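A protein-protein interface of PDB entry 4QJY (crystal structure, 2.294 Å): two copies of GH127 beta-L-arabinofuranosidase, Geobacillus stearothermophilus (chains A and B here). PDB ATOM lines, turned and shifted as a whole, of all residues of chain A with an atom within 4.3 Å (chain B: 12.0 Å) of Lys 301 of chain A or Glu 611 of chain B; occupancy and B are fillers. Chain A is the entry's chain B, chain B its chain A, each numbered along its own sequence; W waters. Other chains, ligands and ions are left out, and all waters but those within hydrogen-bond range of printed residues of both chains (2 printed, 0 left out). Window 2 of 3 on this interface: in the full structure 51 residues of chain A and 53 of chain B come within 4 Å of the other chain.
OE1 of Glu 611 of chain B lies within salt-bridge range of NZ of Lys 301 of chain A, 3.9 Å away. N of His 540 of chain A sits at hydrogen-bond distance from O of Leu 612 of chain B, at 2.9 Å. The indole nitrogen of Trp 608 of chain B sits close to the backbone NH of His 540 of chain A, 3.4 Å away.
No residue of chain B comes within 4 Å of Glu 297 of chain A. No residue of chain B comes within 4 Å of Asn 298 of chain A. Val 299 of chain A touches none of the printed residues of chain B. Of chain B, only Asp 610 (3.1 Å), Glu 611 (3.9 Å) and Leu 612 (3.5 Å) come within 4 Å of Lys 301 of chain A. Of chain B, only Leu 612 (3.8 Å) comes within 4 Å of Arg 302 of chain A. His 540 of chain A touches four residues of chain B. Val 603 of chain B touches none of the printed residues of chain A. Of the printed residues of chain A, Trp 608 of chain B touches His 540. Asn 609 of chain B touches none of the printed residues of chain A. Of the printed residues of chain A, Asp 610 of chain B touches Lys 301 (3.1 Å). Of chain A, only Lys 301 (3.9 Å) and His 540 (3.4 Å) come within 4 Å of Glu 611 of chain B. Printed residues of chain A within 4 Å of Leu 612 of chain B: Thr 300 (3.5 Å), Lys 301 (3.5 Å), Arg 302 (3.8 Å) and His 540 (2.9 Å). The nearest residue of chain B that does not touch Lys 301 of chain A is Asn 609 of chain B (5.6 Å). The nearest printed residue of chain A that does not touch Glu 605 of chain B is Phe 323 of chain A (6.7 Å).
NH1 of Arg 614 of chain B is in hydrogen-bond range of O of Trp 608 of chain B, at 3.1 Å. OE2 of Glu 297 of chain A is in salt-bridge range of NZ of Lys 301 of chain A, 3.1 Å away. The backbone carbonyl oxygen (O) of Arg 302 of chain A lies within hydrogen-bond range of the backbone NH (N) of Phe 323 of chain A (2.8 Å).
Water W1 lies within hydrogen-bond range of NH1 of Arg 302 of chain A, O of Asp 610 of chain B and O of Lys 301 of chain A. Water W2 lies within hydrogen-bond range of the backbone carbonyl oxygen of Thr 300 of chain A (2.9 Å) and the backbone NH of Leu 612 of chain B (3.3 Å).
Thr 300 of chain A touches Leu 612 of chain B. Lys 301 of chain A touches Asp 610 of chain B. Leu 612 of chain B touches Lys 301 of chain A. Arg 302 of chain A touches Leu 612 of chain B (N to CD2, 3.8 Å). His 540 of chain A touches Glu 605 of chain B. CD2 of His 540 of chain A touches O of Glu 611 of chain B, 3.4 Å away.
No position is printed for both chains. Of the 9 pairs that touch across the chains among the printed residues, none has its exchanged pair printed and touching as well.
Of the 17 printed residues of chain B, 5 touch a printed residue of chain A. Of the 9 printed residues of chain A, 4 touch a printed residue of chain B. Hydrophobic or aromatic side chains of chain A that line the printed part of chain B: His 540.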
ATOM      1  N   GLU A 297      21.404  28.565 -28.374  1.00  0.00           N
ATOM      2  CA  GLU A 297      22.051  27.269 -28.249  1.00  0.00           C
ATOM      3  C   GLU A 297      21.474  26.537 -27.038  1.00  0.00           C
ATOM      4  O   GLU A 297      21.112  25.352 -27.116  1.00  0.00           O
ATOM      5  CB  GLU A 297      23.577  27.355 -28.174  1.00  0.00           C
ATOM      6  CG  GLU A 297      24.316  27.888 -29.445  1.00  0.00           C
ATOM      7  CD  GLU A 297      24.294  26.981 -30.725  1.00  0.00           C
ATOM      8  OE1 GLU A 297      25.327  26.314 -31.019  1.00  0.00           O
ATOM      9  OE2 GLU A 297      23.296  26.950 -31.494  1.00  0.00           O
ATOM     10  N   ASN A 298      21.310  27.264 -25.937  1.00  0.00           N
ATOM     11  CA  ASN A 298      20.789  26.670 -24.748  1.00  0.00           C
ATOM     12  C   ASN A 298      19.387  26.138 -24.975  1.00  0.00           C
ATOM     13  O   ASN A 298      19.090  25.017 -24.576  1.00  0.00           O
ATOM     14  CB  ASN A 298      20.793  27.646 -23.577  1.00  0.00           C
ATOM     15  CG  ASN A 298      20.425  26.979 -22.258  1.00  0.00           C
ATOM     16  OD1 ASN A 298      19.462  27.333 -21.644  1.00  0.00           O
ATOM     17  ND2 ASN A 298      21.203  25.998 -21.838  1.00  0.00           N
ATOM     18  N   VAL A 299      18.519  26.932 -25.586  1.00  0.00           N
ATOM     19  CA  VAL A 299      17.143  26.508 -25.743  1.00  0.00           C
ATOM     20  C   VAL A 299      17.045  25.303 -26.679  1.00  0.00           C
ATOM     21  O   VAL A 299      16.410  24.281 -26.372  1.00  0.00           O
ATOM     22  CB  VAL A 299      16.249  27.633 -26.241  1.00  0.00           C
ATOM     23  CG1 VAL A 299      14.867  27.090 -26.617  1.00  0.00           C
ATOM     24  CG2 VAL A 299      16.045  28.710 -25.155  1.00  0.00           C
ATOM     25  N   THR A 300      17.669  25.431 -27.841  1.00  0.00           N
ATOM     26  CA  THR A 300      17.376  24.529 -28.955  1.00  0.00           C
ATOM     27  C   THR A 300      18.252  23.301 -28.930  1.00  0.00           C
ATOM     28  O   THR A 300      17.923  22.349 -29.582  1.00  0.00           O
ATOM     29  CB  THR A 300      17.478  25.213 -30.323  1.00  0.00           C
ATOM     30  OG1 THR A 300      18.793  25.708 -30.523  1.00  0.00           O
ATOM     31  CG2 THR A 300      16.493  26.342 -30.389  1.00  0.00           C
ATOM     32  N   LYS A 301      19.346  23.338 -28.176  1.00  0.00           N
ATOM     33  CA  LYS A 301      20.190  22.177 -27.974  1.00  0.00           C
ATOM     34  C   LYS A 301      20.163  21.579 -26.603  1.00  0.00           C
ATOM     35  O   LYS A 301      20.867  20.591 -26.381  1.00  0.00           O
ATOM     36  CB  LYS A 301      21.628  22.532 -28.272  1.00  0.00           C
ATOM     37  CG  LYS A 301      21.857  23.009 -29.713  1.00  0.00           C
ATOM     38  CD  LYS A 301      23.263  22.635 -30.161  1.00  0.00           C
ATOM     39  CE  LYS A 301      23.925  23.699 -31.013  1.00  0.00           C
ATOM     40  NZ  LYS A 301      23.174  23.960 -32.280  1.00  0.00           N
ATOM     41  N   ARG A 302      19.409  22.177 -25.670  1.00  0.00           N
ATOM     42  CA  ARG A 302      19.260  21.605 -24.316  1.00  0.00           C
ATOM     43  C   ARG A 302      17.870  21.533 -23.722  1.00  0.00           C
ATOM     44  O   ARG A 302      17.685  20.742 -22.856  1.00  0.00           O
ATOM     45  CB  ARG A 302      20.074  22.352 -23.282  1.00  0.00           C
ATOM     46  CG  ARG A 302      21.475  22.672 -23.654  1.00  0.00           C
ATOM     47  CD  ARG A 302      22.296  21.459 -23.803  1.00  0.00           C
ATOM     48  NE  ARG A 302      23.599  21.742 -23.269  1.00  0.00           N
ATOM     49  CZ  ARG A 302      24.738  21.387 -23.850  1.00  0.00           C
ATOM     50  NH1 ARG A 302      24.733  20.701 -25.001  1.00  0.00           N
ATOM     51  NH2 ARG A 302      25.894  21.719 -23.256  1.00  0.00           N
ATOM     52  N   GLN A 303      16.936  22.368 -24.156  1.00  0.00           N
ATOM     53  CA  GLN A 303      15.620  22.510 -23.507  1.00  0.00           C
ATOM     54  C   GLN A 303      14.428  22.588 -24.490  1.00  0.00           C
ATOM     55  O   GLN A 303      13.488  23.346 -24.273  1.00  0.00           O
ATOM     56  CB  GLN A 303      15.616  23.771 -22.636  1.00  0.00           C
ATOM     57  CG  GLN A 303      16.715  23.798 -21.580  1.00  0.00           C
ATOM     58  CD  GLN A 303      16.410  24.747 -20.412  1.00  0.00           C
ATOM     59  OE1 GLN A 303      15.442  24.566 -19.670  1.00  0.00           O
ATOM     60  NE2 GLN A 303      17.208  25.781 -20.278  1.00  0.00           N
ATOM     61  N   PHE A 323      18.600  19.296 -20.688  1.00  0.00           N
ATOM     62  CA  PHE A 323      18.373  17.870 -20.931  1.00  0.00           C
ATOM     63  C   PHE A 323      17.216  17.259 -20.181  1.00  0.00           C
ATOM     64  O   PHE A 323      17.000  16.049 -20.278  1.00  0.00           O
ATOM     65  CB  PHE A 323      19.636  17.061 -20.662  1.00  0.00           C
ATOM     66  CG  PHE A 323      20.842  17.500 -21.494  1.00  0.00           C
ATOM     67  CD1 PHE A 323      20.826  17.374 -22.872  1.00  0.00           C
ATOM     68  CD2 PHE A 323      21.979  18.015 -20.876  1.00  0.00           C
ATOM     69  CE1 PHE A 323      21.900  17.749 -23.619  1.00  0.00           C
ATOM     70  CE2 PHE A 323      23.091  18.371 -21.614  1.00  0.00           C
ATOM     71  CZ  PHE A 323      23.060  18.227 -22.981  1.00  0.00           C
ATOM     72  N   HIS A 540      20.069  12.919 -27.744  1.00  0.00           N
ATOM     73  CA  HIS A 540      21.337  12.928 -27.022  1.00  0.00           C
ATOM     74  C   HIS A 540      21.243  12.064 -25.762  1.00  0.00           C
ATOM     75  O   HIS A 540      20.265  12.116 -25.037  1.00  0.00           O
ATOM     76  CB  HIS A 540      21.657  14.372 -26.666  1.00  0.00           C
ATOM     77  CG  HIS A 540      23.077  14.614 -26.286  1.00  0.00           C
ATOM     78  ND1 HIS A 540      23.613  14.199 -25.075  1.00  0.00           N
ATOM     79  CD2 HIS A 540      24.068  15.274 -26.931  1.00  0.00           C
ATOM     80  CE1 HIS A 540      24.869  14.595 -25.002  1.00  0.00           C
ATOM     81  NE2 HIS A 540      25.172  15.236 -26.116  1.00  0.00           N
ATOM     82  N   TRP B 388      17.718  11.291  -9.984  1.00  0.00           N
ATOM     83  CA  TRP B 388      18.664  12.226 -10.656  1.00  0.00           C
ATOM     84  C   TRP B 388      18.711  13.482  -9.804  1.00  0.00           C
ATOM     85  O   TRP B 388      17.771  14.226  -9.820  1.00  0.00           O
ATOM     86  CB  TRP B 388      18.167  12.510 -12.065  1.00  0.00           C
ATOM     87  CG  TRP B 388      19.034  13.406 -12.878  1.00  0.00           C
ATOM     88  CD1 TRP B 388      20.330  13.778 -12.623  1.00  0.00           C
ATOM     89  CD2 TRP B 388      18.677  14.014 -14.127  1.00  0.00           C
ATOM     90  NE1 TRP B 388      20.781  14.587 -13.631  1.00  0.00           N
ATOM     91  CE2 TRP B 388      19.801  14.731 -14.573  1.00  0.00           C
ATOM     92  CE3 TRP B 388      17.504  14.021 -14.906  1.00  0.00           C
ATOM     93  CZ2 TRP B 388      19.784  15.481 -15.735  1.00  0.00           C
ATOM     94  CZ3 TRP B 388      17.484  14.754 -16.096  1.00  0.00           C
ATOM     95  CH2 TRP B 388      18.611  15.485 -16.486  1.00  0.00           C
ATOM     96  N   ASN B 569      24.848   9.551 -15.249  1.00  0.00           N
ATOM     97  CA  ASN B 569      23.944   9.136 -16.299  1.00  0.00           C
ATOM     98  C   ASN B 569      23.648   7.620 -16.370  1.00  0.00           C
ATOM     99  O   ASN B 569      23.954   6.947 -17.323  1.00  0.00           O
ATOM    100  CB  ASN B 569      24.341   9.676 -17.696  1.00  0.00           C
ATOM    101  CG  ASN B 569      23.115   9.692 -18.656  1.00  0.00           C
ATOM    102  OD1 ASN B 569      22.051   9.173 -18.309  1.00  0.00           O
ATOM    103  ND2 ASN B 569      23.237  10.337 -19.805  1.00  0.00           N
ATOM    104  N   VAL B 603      26.004   4.387 -24.383  1.00  0.00           N
ATOM    105  CA  VAL B 603      26.103   5.043 -25.656  1.00  0.00           C
ATOM    106  C   VAL B 603      27.157   6.115 -25.577  1.00  0.00           C
ATOM    107  O   VAL B 603      27.194   6.846 -24.583  1.00  0.00           O
ATOM    108  CB  VAL B 603      24.793   5.640 -26.086  1.00  0.00           C
ATOM    109  CG1 VAL B 603      25.003   6.371 -27.390  1.00  0.00           C
ATOM    110  CG2 VAL B 603      23.756   4.534 -26.244  1.00  0.00           C
ATOM    111  N   ASP B 604      28.007   6.203 -26.609  1.00  0.00           N
ATOM    112  CA  ASP B 604      29.000   7.298 -26.765  1.00  0.00           C
ATOM    113  C   ASP B 604      28.379   8.606 -27.322  1.00  0.00           C
ATOM    114  O   ASP B 604      27.806   8.623 -28.387  1.00  0.00           O
ATOM    115  CB  ASP B 604      30.129   6.840 -27.673  1.00  0.00           C
ATOM    116  CG  ASP B 604      31.227   7.935 -27.896  1.00  0.00           C
ATOM    117  OD1 ASP B 604      31.096   9.062 -27.436  1.00  0.00           O
ATOM    118  OD2 ASP B 604      32.242   7.648 -28.559  1.00  0.00           O
ATOM    119  N   GLU B 605      28.549   9.712 -26.617  1.00  0.00           N
ATOM    120  CA  GLU B 605      27.794  10.944 -26.879  1.00  0.00           C
ATOM    121  C   GLU B 605      28.308  11.730 -28.105  1.00  0.00           C
ATOM    122  O   GLU B 605      27.533  12.408 -28.824  1.00  0.00           O
ATOM    123  CB  GLU B 605      27.865  11.879 -25.657  1.00  0.00           C
ATOM    124  CG  GLU B 605      28.008  11.224 -24.280  1.00  0.00           C
ATOM    125  CD  GLU B 605      27.512  12.132 -23.165  1.00  0.00           C
ATOM    126  OE1 GLU B 605      26.891  11.623 -22.215  1.00  0.00           O
ATOM    127  OE2 GLU B 605      27.716  13.355 -23.247  1.00  0.00           O
ATOM    128  N   SER B 606      29.613  11.642 -28.330  1.00  0.00           N
ATOM    129  CA  SER B 606      30.287  12.423 -29.361  1.00  0.00           C
ATOM    130  C   SER B 606      29.651  12.425 -30.762  1.00  0.00           C
ATOM    131  O   SER B 606      29.703  13.454 -31.425  1.00  0.00           O
ATOM    132  CB  SER B 606      31.755  12.009 -29.436  1.00  0.00           C
ATOM    133  OG  SER B 606      31.882  10.625 -29.594  1.00  0.00           O
ATOM    134  N   ALA B 607      29.004  11.338 -31.201  1.00  0.00           N
ATOM    135  CA  ALA B 607      28.289  11.347 -32.525  1.00  0.00           C
ATOM    136  C   ALA B 607      27.131  12.361 -32.690  1.00  0.00           C
ATOM    137  O   ALA B 607      26.681  12.670 -33.838  1.00  0.00           O
ATOM    138  CB  ALA B 607      27.782   9.966 -32.871  1.00  0.00           C
ATOM    139  N   TRP B 608      26.626  12.860 -31.564  1.00  0.00           N
ATOM    140  CA  TRP B 608      25.650  13.958 -31.601  1.00  0.00           C
ATOM    141  C   TRP B 608      26.273  15.343 -32.017  1.00  0.00           C
ATOM    142  O   TRP B 608      25.538  16.194 -32.532  1.00  0.00           O
ATOM    143  CB  TRP B 608      24.853  14.034 -30.280  1.00  0.00           C
ATOM    144  CG  TRP B 608      23.721  13.055 -30.295  1.00  0.00           C
ATOM    145  CD1 TRP B 608      22.422  13.297 -30.660  1.00  0.00           C
ATOM    146  CD2 TRP B 608      23.807  11.656 -30.047  1.00  0.00           C
ATOM    147  NE1 TRP B 608      21.690  12.125 -30.643  1.00  0.00           N
ATOM    148  CE2 TRP B 608      22.513  11.110 -30.243  1.00  0.00           C
ATOM    149  CE3 TRP B 608      24.832  10.817 -29.627  1.00  0.00           C
ATOM    150  CZ2 TRP B 608      22.238   9.788 -30.047  1.00  0.00           C
ATOM    151  CZ3 TRP B 608      24.548   9.500 -29.429  1.00  0.00           C
ATOM    152  CH2 TRP B 608      23.271   8.992 -29.646  1.00  0.00           C
ATOM    153  N   ASN B 609      27.590  15.544 -31.838  1.00  0.00           N
ATOM    154  CA  ASN B 609      28.235  16.865 -32.064  1.00  0.00           C
ATOM    155  C   ASN B 609      27.449  17.969 -31.350  1.00  0.00           C
ATOM    156  O   ASN B 609      27.126  19.003 -31.937  1.00  0.00           O
ATOM    157  CB  ASN B 609      28.360  17.208 -33.569  1.00  0.00           C
ATOM    158  CG  ASN B 609      29.273  16.234 -34.334  1.00  0.00           C
ATOM    159  OD1 ASN B 609      30.360  15.858 -33.857  1.00  0.00           O
ATOM    160  ND2 ASN B 609      28.831  15.820 -35.533  1.00  0.00           N
ATOM    161  N   ASP B 610      27.072  17.695 -30.103  1.00  0.00           N
ATOM    162  CA  ASP B 610      26.314  18.649 -29.277  1.00  0.00           C
ATOM    163  C   ASP B 610      24.907  18.967 -29.791  1.00  0.00           C
ATOM    164  O   ASP B 610      24.215  19.802 -29.217  1.00  0.00           O
ATOM    165  CB  ASP B 610      27.135  19.926 -29.046  1.00  0.00           C
ATOM    166  CG  ASP B 610      28.507  19.614 -28.406  1.00  0.00           C
ATOM    167  OD1 ASP B 610      28.524  19.143 -27.236  1.00  0.00           O
ATOM    168  OD2 ASP B 610      29.566  19.817 -29.070  1.00  0.00           O
ATOM    169  N   GLU B 611      24.476  18.286 -30.847  1.00  0.00           N
ATOM    170  CA  GLU B 611      23.077  18.341 -31.286  1.00  0.00           C
ATOM    171  C   GLU B 611      22.164  17.498 -30.372  1.00  0.00           C
ATOM    172  O   GLU B 611      22.595  16.539 -29.750  1.00  0.00           O
ATOM    173  CB  GLU B 611      22.948  17.870 -32.738  1.00  0.00           C
ATOM    174  CG  GLU B 611      22.056  18.767 -33.593  1.00  0.00           C
ATOM    175  CD  GLU B 611      22.782  19.944 -34.240  1.00  0.00           C
ATOM    176  OE1 GLU B 611      23.846  20.389 -33.739  1.00  0.00           O
ATOM    177  OE2 GLU B 611      22.268  20.441 -35.256  1.00  0.00           O
ATOM    178  N   LEU B 612      20.907  17.871 -30.306  1.00  0.00           N
ATOM    179  CA  LEU B 612      19.930  17.210 -29.461  1.00  0.00           C
ATOM    180  C   LEU B 612      19.251  16.012 -30.135  1.00  0.00           C
ATOM    181  O   LEU B 612      19.049  14.984 -29.512  1.00  0.00           O
ATOM    182  CB  LEU B 612      18.864  18.230 -29.105  1.00  0.00           C
ATOM    183  CG  LEU B 612      18.052  18.142 -27.855  1.00  0.00           C
ATOM    184  CD1 LEU B 612      18.890  17.752 -26.657  1.00  0.00           C
ATOM    185  CD2 LEU B 612      17.428  19.521 -27.625  1.00  0.00           C
ATOM    186  N   TYR B 613      18.869  16.157 -31.396  1.00  0.00           N
ATOM    187  CA  TYR B 613      18.134  15.123 -32.091  1.00  0.00           C
ATOM    188  C   TYR B 613      18.803  14.757 -33.419  1.00  0.00           C
ATOM    189  O   TYR B 613      19.026  15.627 -34.258  1.00  0.00           O
ATOM    190  CB  TYR B 613      16.722  15.594 -32.303  1.00  0.00           C
ATOM    191  CG  TYR B 613      16.045  15.990 -31.043  1.00  0.00           C
ATOM    192  CD1 TYR B 613      15.890  15.084 -30.013  1.00  0.00           C
ATOM    193  CD2 TYR B 613      15.549  17.257 -30.858  1.00  0.00           C
ATOM    194  CE1 TYR B 613      15.294  15.451 -28.811  1.00  0.00           C
ATOM    195  CE2 TYR B 613      14.925  17.629 -29.671  1.00  0.00           C
ATOM    196  CZ  TYR B 613      14.812  16.723 -28.646  1.00  0.00           C
ATOM    197  OH  TYR B 613      14.214  17.054 -27.471  1.00  0.00           O
ATOM    198  N   ARG B 614      19.116  13.491 -33.621  1.00  0.00           N
ATOM    199  CA  ARG B 614      19.830  13.065 -34.844  1.00  0.00           C
ATOM    200  C   ARG B 614      19.443  11.650 -35.247  1.00  0.00           C
ATOM    201  O   ARG B 614      19.256  10.796 -34.398  1.00  0.00           O
ATOM    202  CB  ARG B 614      21.346  13.057 -34.647  1.00  0.00           C
ATOM    203  CG  ARG B 614      21.996  14.415 -34.475  1.00  0.00           C
ATOM    204  CD  ARG B 614      22.109  15.171 -35.787  1.00  0.00           C
ATOM    205  NE  ARG B 614      23.155  14.571 -36.612  1.00  0.00           N
ATOM    206  CZ  ARG B 614      24.471  14.755 -36.454  1.00  0.00           C
ATOM    207  NH1 ARG B 614      24.958  15.562 -35.517  1.00  0.00           N
ATOM    208  NH2 ARG B 614      25.308  14.132 -37.267  1.00  0.00           N
ATOM    209  N   PRO B 615      19.388  11.393 -36.556  1.00  0.00           N
ATOM    210  CA  PRO B 615      19.135  10.083 -37.081  1.00  0.00           C
ATOM    211  C   PRO B 615      20.418   9.275 -37.150  1.00  0.00           C
ATOM    212  O   PRO B 615      20.878   8.987 -38.220  1.00  0.00           O
ATOM    213  CB  PRO B 615      18.611  10.402 -38.484  1.00  0.00           C
ATOM    214  CG  PRO B 615      19.437  11.582 -38.900  1.00  0.00           C
ATOM    215  CD  PRO B 615      19.594  12.379 -37.643  1.00  0.00           C
ATOM    216  N   ILE B 616      20.997   8.910 -36.029  1.00  0.00           N
ATOM    217  CA  ILE B 616      22.239   8.139 -36.055  1.00  0.00           C
ATOM    218  C   ILE B 616      22.126   6.731 -35.443  1.00  0.00           C
ATOM    219  O   ILE B 616      21.279   6.474 -34.609  1.00  0.00           O
ATOM    220  CB  ILE B 616      23.398   8.904 -35.368  1.00  0.00           C
ATOM    221  CG1 ILE B 616      23.088   9.162 -33.914  1.00  0.00           C
ATOM    222  CG2 ILE B 616      23.652  10.234 -36.080  1.00  0.00           C
ATOM    223  CD1 ILE B 616      23.673   8.110 -33.030  1.00  0.00           C
ATOM    224  N   PRO B 618      23.873   4.606 -32.981  1.00  0.00           N
ATOM    225  CA  PRO B 618      24.806   4.983 -31.954  1.00  0.00           C
ATOM    226  C   PRO B 618      25.847   3.905 -31.733  1.00  0.00           C
ATOM    227  O   PRO B 618      25.528   2.703 -31.762  1.00  0.00           O
ATOM    228  CB  PRO B 618      23.917   5.150 -30.729  1.00  0.00           C
ATOM    229  CG  PRO B 618      22.791   4.194 -30.939  1.00  0.00           C
ATOM    230  CD  PRO B 618      22.614   4.066 -32.437  1.00  0.00           C
HETATM  231  O   HOH W   1      23.359  19.561 -26.726  1.00  0.00           O
HETATM  232  O   HOH W   2      19.481  20.639 -31.395  1.00  0.00           O
